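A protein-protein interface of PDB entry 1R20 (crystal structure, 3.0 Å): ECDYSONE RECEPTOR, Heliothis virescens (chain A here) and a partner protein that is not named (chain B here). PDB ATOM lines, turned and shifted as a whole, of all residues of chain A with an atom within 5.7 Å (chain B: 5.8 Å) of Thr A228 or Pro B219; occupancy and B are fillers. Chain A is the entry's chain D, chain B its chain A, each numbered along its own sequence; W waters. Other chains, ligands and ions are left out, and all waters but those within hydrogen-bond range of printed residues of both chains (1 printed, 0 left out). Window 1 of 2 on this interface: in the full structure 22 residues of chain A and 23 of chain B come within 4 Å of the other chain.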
ATOM      1  N   SER A 180      23.262   7.496   2.100  1.00  0.00           N
ATOM      2  CA  SER A 180      23.280   7.801   0.685  1.00  0.00           C
ATOM      3  C   SER A 180      23.905   9.208   0.695  1.00  0.00           C
ATOM      4  O   SER A 180      23.556  10.032   1.554  1.00  0.00           O
ATOM      5  CB  SER A 180      21.837   7.862   0.158  1.00  0.00           C
ATOM      6  OG  SER A 180      21.713   7.447  -1.202  1.00  0.00           O
ATOM      7  N   LEU A 224      19.614  -1.818  -5.236  1.00  0.00           N
ATOM      8  CA  LEU A 224      20.143  -0.479  -5.456  1.00  0.00           C
ATOM      9  C   LEU A 224      19.237   0.253  -6.441  1.00  0.00           C
ATOM     10  O   LEU A 224      19.136   1.458  -6.460  1.00  0.00           O
ATOM     11  CB  LEU A 224      21.556  -0.588  -6.016  1.00  0.00           C
ATOM     12  CG  LEU A 224      22.487  -1.444  -5.109  1.00  0.00           C
ATOM     13  CD1 LEU A 224      23.798  -1.831  -5.842  1.00  0.00           C
ATOM     14  CD2 LEU A 224      22.746  -0.682  -3.761  1.00  0.00           C
ATOM     15  N   GLY A 225      18.534  -0.517  -7.246  1.00  0.00           N
ATOM     16  CA  GLY A 225      17.682   0.055  -8.259  1.00  0.00           C
ATOM     17  C   GLY A 225      16.559   0.843  -7.670  1.00  0.00           C
ATOM     18  O   GLY A 225      15.980   1.687  -8.362  1.00  0.00           O
ATOM     19  N   ILE A 226      16.212   0.545  -6.416  1.00  0.00           N
ATOM     20  CA  ILE A 226      15.127   1.261  -5.715  1.00  0.00           C
ATOM     21  C   ILE A 226      15.639   2.630  -5.336  1.00  0.00           C
ATOM     22  O   ILE A 226      15.013   3.613  -5.642  1.00  0.00           O
ATOM     23  CB  ILE A 226      14.718   0.591  -4.442  1.00  0.00           C
ATOM     24  CG1 ILE A 226      13.711  -0.489  -4.743  1.00  0.00           C
ATOM     25  CG2 ILE A 226      14.194   1.626  -3.497  1.00  0.00           C
ATOM     26  CD1 ILE A 226      13.100  -1.153  -3.502  1.00  0.00           C
ATOM     27  N   LEU A 227      16.776   2.651  -4.646  1.00  0.00           N
ATOM     28  CA  LEU A 227      17.459   3.854  -4.233  1.00  0.00           C
ATOM     29  C   LEU A 227      17.296   4.951  -5.309  1.00  0.00           C
ATOM     30  O   LEU A 227      17.058   6.128  -5.001  1.00  0.00           O
ATOM     31  CB  LEU A 227      18.908   3.529  -4.076  1.00  0.00           C
ATOM     32  CG  LEU A 227      19.590   3.911  -2.816  1.00  0.00           C
ATOM     33  CD1 LEU A 227      19.408   2.762  -1.884  1.00  0.00           C
ATOM     34  CD2 LEU A 227      21.072   4.207  -3.079  1.00  0.00           C
ATOM     35  N   THR A 228      17.432   4.617  -6.583  1.00  0.00           N
ATOM     36  CA  THR A 228      17.215   5.679  -7.551  1.00  0.00           C
ATOM     37  C   THR A 228      15.725   6.163  -7.658  1.00  0.00           C
ATOM     38  O   THR A 228      15.477   7.355  -7.854  1.00  0.00           O
ATOM     39  CB  THR A 228      17.766   5.309  -8.958  1.00  0.00           C
ATOM     40  OG1 THR A 228      17.234   6.224  -9.885  1.00  0.00           O
ATOM     41  CG2 THR A 228      17.309   3.972  -9.437  1.00  0.00           C
ATOM     42  N   GLU A 229      14.738   5.272  -7.528  1.00  0.00           N
ATOM     43  CA  GLU A 229      13.319   5.684  -7.624  1.00  0.00           C
ATOM     44  C   GLU A 229      12.752   6.380  -6.359  1.00  0.00           C
ATOM     45  O   GLU A 229      11.769   7.120  -6.397  1.00  0.00           O
ATOM     46  CB  GLU A 229      12.475   4.477  -7.954  1.00  0.00           C
ATOM     47  CG  GLU A 229      11.829   4.571  -9.304  1.00  0.00           C
ATOM     48  CD  GLU A 229      12.825   4.396 -10.458  1.00  0.00           C
ATOM     49  OE1 GLU A 229      13.733   3.524 -10.304  1.00  0.00           O
ATOM     50  OE2 GLU A 229      12.686   5.107 -11.510  1.00  0.00           O
ATOM     51  N   ILE A 230      13.401   6.111  -5.235  1.00  0.00           N
ATOM     52  CA  ILE A 230      13.090   6.661  -3.943  1.00  0.00           C
ATOM     53  C   ILE A 230      13.431   8.162  -4.043  1.00  0.00           C
ATOM     54  O   ILE A 230      12.855   8.970  -3.335  1.00  0.00           O
ATOM     55  CB  ILE A 230      13.984   5.959  -2.901  1.00  0.00           C
ATOM     56  CG1 ILE A 230      13.167   5.471  -1.730  1.00  0.00           C
ATOM     57  CG2 ILE A 230      15.085   6.885  -2.409  1.00  0.00           C
ATOM     58  CD1 ILE A 230      14.035   5.193  -0.461  1.00  0.00           C
ATOM     59  N   ARG A 231      14.370   8.544  -4.918  1.00  0.00           N
ATOM     60  CA  ARG A 231      14.744   9.957  -5.064  1.00  0.00           C
ATOM     61  C   ARG A 231      13.719  10.778  -5.753  1.00  0.00           C
ATOM     62  O   ARG A 231      13.594  11.933  -5.445  1.00  0.00           O
ATOM     63  CB  ARG A 231      16.014  10.157  -5.863  1.00  0.00           C
ATOM     64  CG  ARG A 231      17.292   9.676  -5.220  1.00  0.00           C
ATOM     65  CD  ARG A 231      17.733  10.473  -4.000  1.00  0.00           C
ATOM     66  NE  ARG A 231      18.990   9.903  -3.567  1.00  0.00           N
ATOM     67  CZ  ARG A 231      20.158  10.281  -4.050  1.00  0.00           C
ATOM     68  NH1 ARG A 231      20.198  11.241  -4.952  1.00  0.00           N
ATOM     69  NH2 ARG A 231      21.272   9.674  -3.666  1.00  0.00           N
ATOM     70  N   THR A 232      13.013  10.210  -6.721  1.00  0.00           N
ATOM     71  CA  THR A 232      11.981  10.968  -7.436  1.00  0.00           C
ATOM     72  C   THR A 232      10.816  11.264  -6.522  1.00  0.00           C
ATOM     73  O   THR A 232      10.284  12.378  -6.516  1.00  0.00           O
ATOM     74  CB  THR A 232      11.407  10.197  -8.616  1.00  0.00           C
ATOM     75  OG1 THR A 232      12.118  10.535  -9.803  1.00  0.00           O
ATOM     76  CG2 THR A 232       9.968  10.529  -8.809  1.00  0.00           C
ATOM     77  N   GLU B  85      17.770  12.159 -18.415  1.00  0.00           N
ATOM     78  CA  GLU B  85      18.842  11.628 -17.558  1.00  0.00           C
ATOM     79  C   GLU B  85      19.980  11.187 -18.490  1.00  0.00           C
ATOM     80  O   GLU B  85      21.140  11.396 -18.196  1.00  0.00           O
ATOM     81  CB  GLU B  85      18.433  10.397 -16.715  1.00  0.00           C
ATOM     82  CG  GLU B  85      17.155  10.463 -15.844  1.00  0.00           C
ATOM     83  CD  GLU B  85      16.799   9.106 -15.096  1.00  0.00           C
ATOM     84  OE1 GLU B  85      17.598   8.656 -14.207  1.00  0.00           O
ATOM     85  OE2 GLU B  85      15.717   8.485 -15.380  1.00  0.00           O
ATOM     86  N   ARG B 189      16.624  -5.498 -18.447  1.00  0.00           N
ATOM     87  CA  ARG B 189      17.436  -4.894 -17.390  1.00  0.00           C
ATOM     88  C   ARG B 189      18.261  -5.916 -16.656  1.00  0.00           C
ATOM     89  O   ARG B 189      19.430  -5.712 -16.445  1.00  0.00           O
ATOM     90  CB  ARG B 189      16.598  -4.127 -16.377  1.00  0.00           C
ATOM     91  CG  ARG B 189      17.346  -3.909 -15.075  1.00  0.00           C
ATOM     92  CD  ARG B 189      16.718  -2.854 -14.183  1.00  0.00           C
ATOM     93  NE  ARG B 189      16.955  -1.504 -14.705  1.00  0.00           N
ATOM     94  CZ  ARG B 189      16.797  -0.377 -14.006  1.00  0.00           C
ATOM     95  NH1 ARG B 189      16.399  -0.394 -12.747  1.00  0.00           N
ATOM     96  NH2 ARG B 189      17.056   0.775 -14.563  1.00  0.00           N
ATOM     97  N   LEU B 215      26.515   1.481  -9.801  1.00  0.00           N
ATOM     98  CA  LEU B 215      25.095   1.587  -9.726  1.00  0.00           C
ATOM     99  C   LEU B 215      24.614   2.732  -8.835  1.00  0.00           C
ATOM    100  O   LEU B 215      23.420   3.092  -8.856  1.00  0.00           O
ATOM    101  CB  LEU B 215      24.559   0.256  -9.269  1.00  0.00           C
ATOM    102  CG  LEU B 215      24.448  -0.631 -10.495  1.00  0.00           C
ATOM    103  CD1 LEU B 215      23.757  -1.925 -10.138  1.00  0.00           C
ATOM    104  CD2 LEU B 215      23.626   0.062 -11.563  1.00  0.00           C
ATOM    105  N   LEU B 216      25.548   3.335  -8.099  1.00  0.00           N
ATOM    106  CA  LEU B 216      25.204   4.413  -7.164  1.00  0.00           C
ATOM    107  C   LEU B 216      25.245   5.816  -7.710  1.00  0.00           C
ATOM    108  O   LEU B 216      24.961   6.775  -6.964  1.00  0.00           O
ATOM    109  CB  LEU B 216      26.121   4.404  -5.938  1.00  0.00           C
ATOM    110  CG  LEU B 216      26.082   3.250  -4.962  1.00  0.00           C
ATOM    111  CD1 LEU B 216      27.095   3.531  -3.909  1.00  0.00           C
ATOM    112  CD2 LEU B 216      24.668   3.062  -4.422  1.00  0.00           C
ATOM    113  N   ARG B 217      25.643   5.939  -8.977  1.00  0.00           N
ATOM    114  CA  ARG B 217      25.733   7.222  -9.655  1.00  0.00           C
ATOM    115  C   ARG B 217      24.343   7.432 -10.159  1.00  0.00           C
ATOM    116  O   ARG B 217      23.888   8.558 -10.328  1.00  0.00           O
ATOM    117  CB  ARG B 217      26.717   7.121 -10.798  1.00  0.00           C
ATOM    118  CG  ARG B 217      27.903   8.111 -10.668  1.00  0.00           C
ATOM    119  CD  ARG B 217      28.152   8.653  -9.254  1.00  0.00           C
ATOM    120  NE  ARG B 217      28.636   7.573  -8.418  1.00  0.00           N
ATOM    121  CZ  ARG B 217      28.536   7.529  -7.100  1.00  0.00           C
ATOM    122  NH1 ARG B 217      27.956   8.526  -6.433  1.00  0.00           N
ATOM    123  NH2 ARG B 217      29.018   6.481  -6.466  1.00  0.00           N
ATOM    124  N   LEU B 218      23.656   6.304 -10.343  1.00  0.00           N
ATOM    125  CA  LEU B 218      22.291   6.272 -10.801  1.00  0.00           C
ATOM    126  C   LEU B 218      21.319   7.027  -9.920  1.00  0.00           C
ATOM    127  O   LEU B 218      20.443   7.638 -10.426  1.00  0.00           O
ATOM    128  CB  LEU B 218      21.877   4.841 -11.015  1.00  0.00           C
ATOM    129  CG  LEU B 218      22.055   4.354 -12.452  1.00  0.00           C
ATOM    130  CD1 LEU B 218      23.230   4.980 -13.052  1.00  0.00           C
ATOM    131  CD2 LEU B 218      22.194   2.868 -12.495  1.00  0.00           C
ATOM    132  N   PRO B 219      21.419   6.974  -8.590  1.00  0.00           N
ATOM    133  CA  PRO B 219      20.366   7.831  -8.007  1.00  0.00           C
ATOM    134  C   PRO B 219      20.702   9.332  -8.117  1.00  0.00           C
ATOM    135  O   PRO B 219      19.814  10.170  -8.207  1.00  0.00           O
ATOM    136  CB  PRO B 219      20.276   7.357  -6.552  1.00  0.00           C
ATOM    137  CG  PRO B 219      20.564   5.880  -6.692  1.00  0.00           C
ATOM    138  CD  PRO B 219      21.777   5.888  -7.648  1.00  0.00           C
ATOM    139  N   ALA B 220      21.986   9.670  -8.114  1.00  0.00           N
ATOM    140  CA  ALA B 220      22.412  11.065  -8.245  1.00  0.00           C
ATOM    141  C   ALA B 220      22.052  11.552  -9.658  1.00  0.00           C
ATOM    142  O   ALA B 220      21.500  12.644  -9.856  1.00  0.00           O
ATOM    143  CB  ALA B 220      23.891  11.156  -8.033  1.00  0.00           C
ATOM    144  N   LEU B 221      22.382  10.738 -10.650  1.00  0.00           N
ATOM    145  CA  LEU B 221      22.026  11.094 -11.993  1.00  0.00           C
ATOM    146  C   LEU B 221      20.519  11.476 -12.050  1.00  0.00           C
ATOM    147  O   LEU B 221      20.139  12.358 -12.821  1.00  0.00           O
ATOM    148  CB  LEU B 221      22.350   9.940 -12.967  1.00  0.00           C
ATOM    149  CG  LEU B 221      21.867  10.289 -14.388  1.00  0.00           C
ATOM    150  CD1 LEU B 221      22.308  11.679 -14.780  1.00  0.00           C
ATOM    151  CD2 LEU B 221      22.373   9.307 -15.357  1.00  0.00           C
ATOM    152  N   ARG B 222      19.676  10.836 -11.235  1.00  0.00           N
ATOM    153  CA  ARG B 222      18.238  11.124 -11.251  1.00  0.00           C
ATOM    154  C   ARG B 222      17.864  12.409 -10.564  1.00  0.00           C
ATOM    155  O   ARG B 222      17.009  13.139 -11.036  1.00  0.00           O
ATOM    156  CB  ARG B 222      17.415  10.000 -10.616  1.00  0.00           C
ATOM    157  CG  ARG B 222      15.916  10.312 -10.484  1.00  0.00           C
ATOM    158  CD  ARG B 222      15.100  10.140 -11.809  1.00  0.00           C
ATOM    159  NE  ARG B 222      15.169   8.760 -12.318  1.00  0.00           N
ATOM    160  CZ  ARG B 222      14.399   7.734 -11.937  1.00  0.00           C
ATOM    161  NH1 ARG B 222      13.430   7.892 -11.039  1.00  0.00           N
ATOM    162  NH2 ARG B 222      14.675   6.513 -12.394  1.00  0.00           N
ATOM    163  N   SER B 223      18.499  12.675  -9.431  1.00  0.00           N
ATOM    164  CA  SER B 223      18.222  13.888  -8.651  1.00  0.00           C
ATOM    165  C   SER B 223      18.625  15.013  -9.514  1.00  0.00           C
ATOM    166  O   SER B 223      17.849  15.971  -9.673  1.00  0.00           O
ATOM    167  CB  SER B 223      19.046  13.929  -7.384  1.00  0.00           C
ATOM    168  OG  SER B 223      18.841  12.712  -6.661  1.00  0.00           O
ATOM    169  N   ILE B 224      19.821  14.908 -10.089  1.00  0.00           N
ATOM    170  CA  ILE B 224      20.274  15.967 -10.958  1.00  0.00           C
ATOM    171  C   ILE B 224      19.362  16.051 -12.163  1.00  0.00           C
ATOM    172  O   ILE B 224      19.151  17.109 -12.728  1.00  0.00           O
ATOM    173  CB  ILE B 224      21.705  15.738 -11.415  1.00  0.00           C
ATOM    174  CG1 ILE B 224      22.649  16.030 -10.278  1.00  0.00           C
ATOM    175  CG2 ILE B 224      22.061  16.658 -12.533  1.00  0.00           C
ATOM    176  CD1 ILE B 224      24.005  15.619 -10.613  1.00  0.00           C
HETATM  177  O   HOH W   1      15.092   1.713 -11.409  1.00  0.00           O
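O of Pro B219 lies within hydrogen-bond range of NH1 of Arg A231, 3.4 Å away. NH2 of Arg B222 is in salt-bridge range of OE2 of Glu A229 (2.6 Å). The side-chain hydroxyl (OG1) of Thr A232 sits at hydrogen-bond distance from the guanidinium group (NH1) of Arg B222, at 3.2 Å. OG of Ser B223 is in hydrogen-bond range of NH1 of Arg A231 (2.6 Å).
The guanidinium group of Arg B222 lies within salt-bridge range of the side-chain carboxylate of Glu B85, 3.1 Å away. The side-chain hydroxyl of Ser B223 lies within hydrogen-bond range of the backbone carbonyl oxygen of Pro B219, at 3.1 Å. The guanidinium group (NH2) of Arg A231 is in hydrogen-bond range of the side-chain hydroxyl (OG) of Ser A180 (3.4 Å).
C of Leu A227 touches CG of Pro B219, at 3.7 Å. Thr A228 touches Leu B218. Pro B219 touches Thr A228 (CG to N, 3.4 Å). Arg B222 touches Thr A228 (NH2 to OG1, 3.6 Å). Ala B220 touches Arg A231.
Pro B219 touches three residues of chain A. Printed residues of chain B within 4 Å of Leu A227: Pro B219. Printed residues of chain B within 4 Å of Glu A229: Arg B222. Of the printed residues of chain A, Ser B223 touches Arg A231 (2.6 Å). Of the printed residues of chain B, Arg A231 touches Pro B219, Ala B220 and Ser B223. Of the printed residues of chain A, Arg B222 touches Thr A228, Glu A229 and Thr A232. Ser A180 touches none of the printed residues of chain B.
Hydrophobic or aromatic side chains of chain A that line the printed part of chain B: Leu A227. Of the 12 printed residues of chain B, 5 touch a printed residue of chain A. Among the printed residues, 9 pairs touch across the chains. Among the printed residues, Asp or Glu carboxylates within 4 Å of a Lys or Arg side-chain nitrogen of the other chain: Glu A229 with Arg B222.
Water W1 lies within hydrogen-bond range of the side-chain carboxylate of Glu A229, the guanidinium group of Arg B189 and the backbone carbonyl oxygen of Gly A225.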
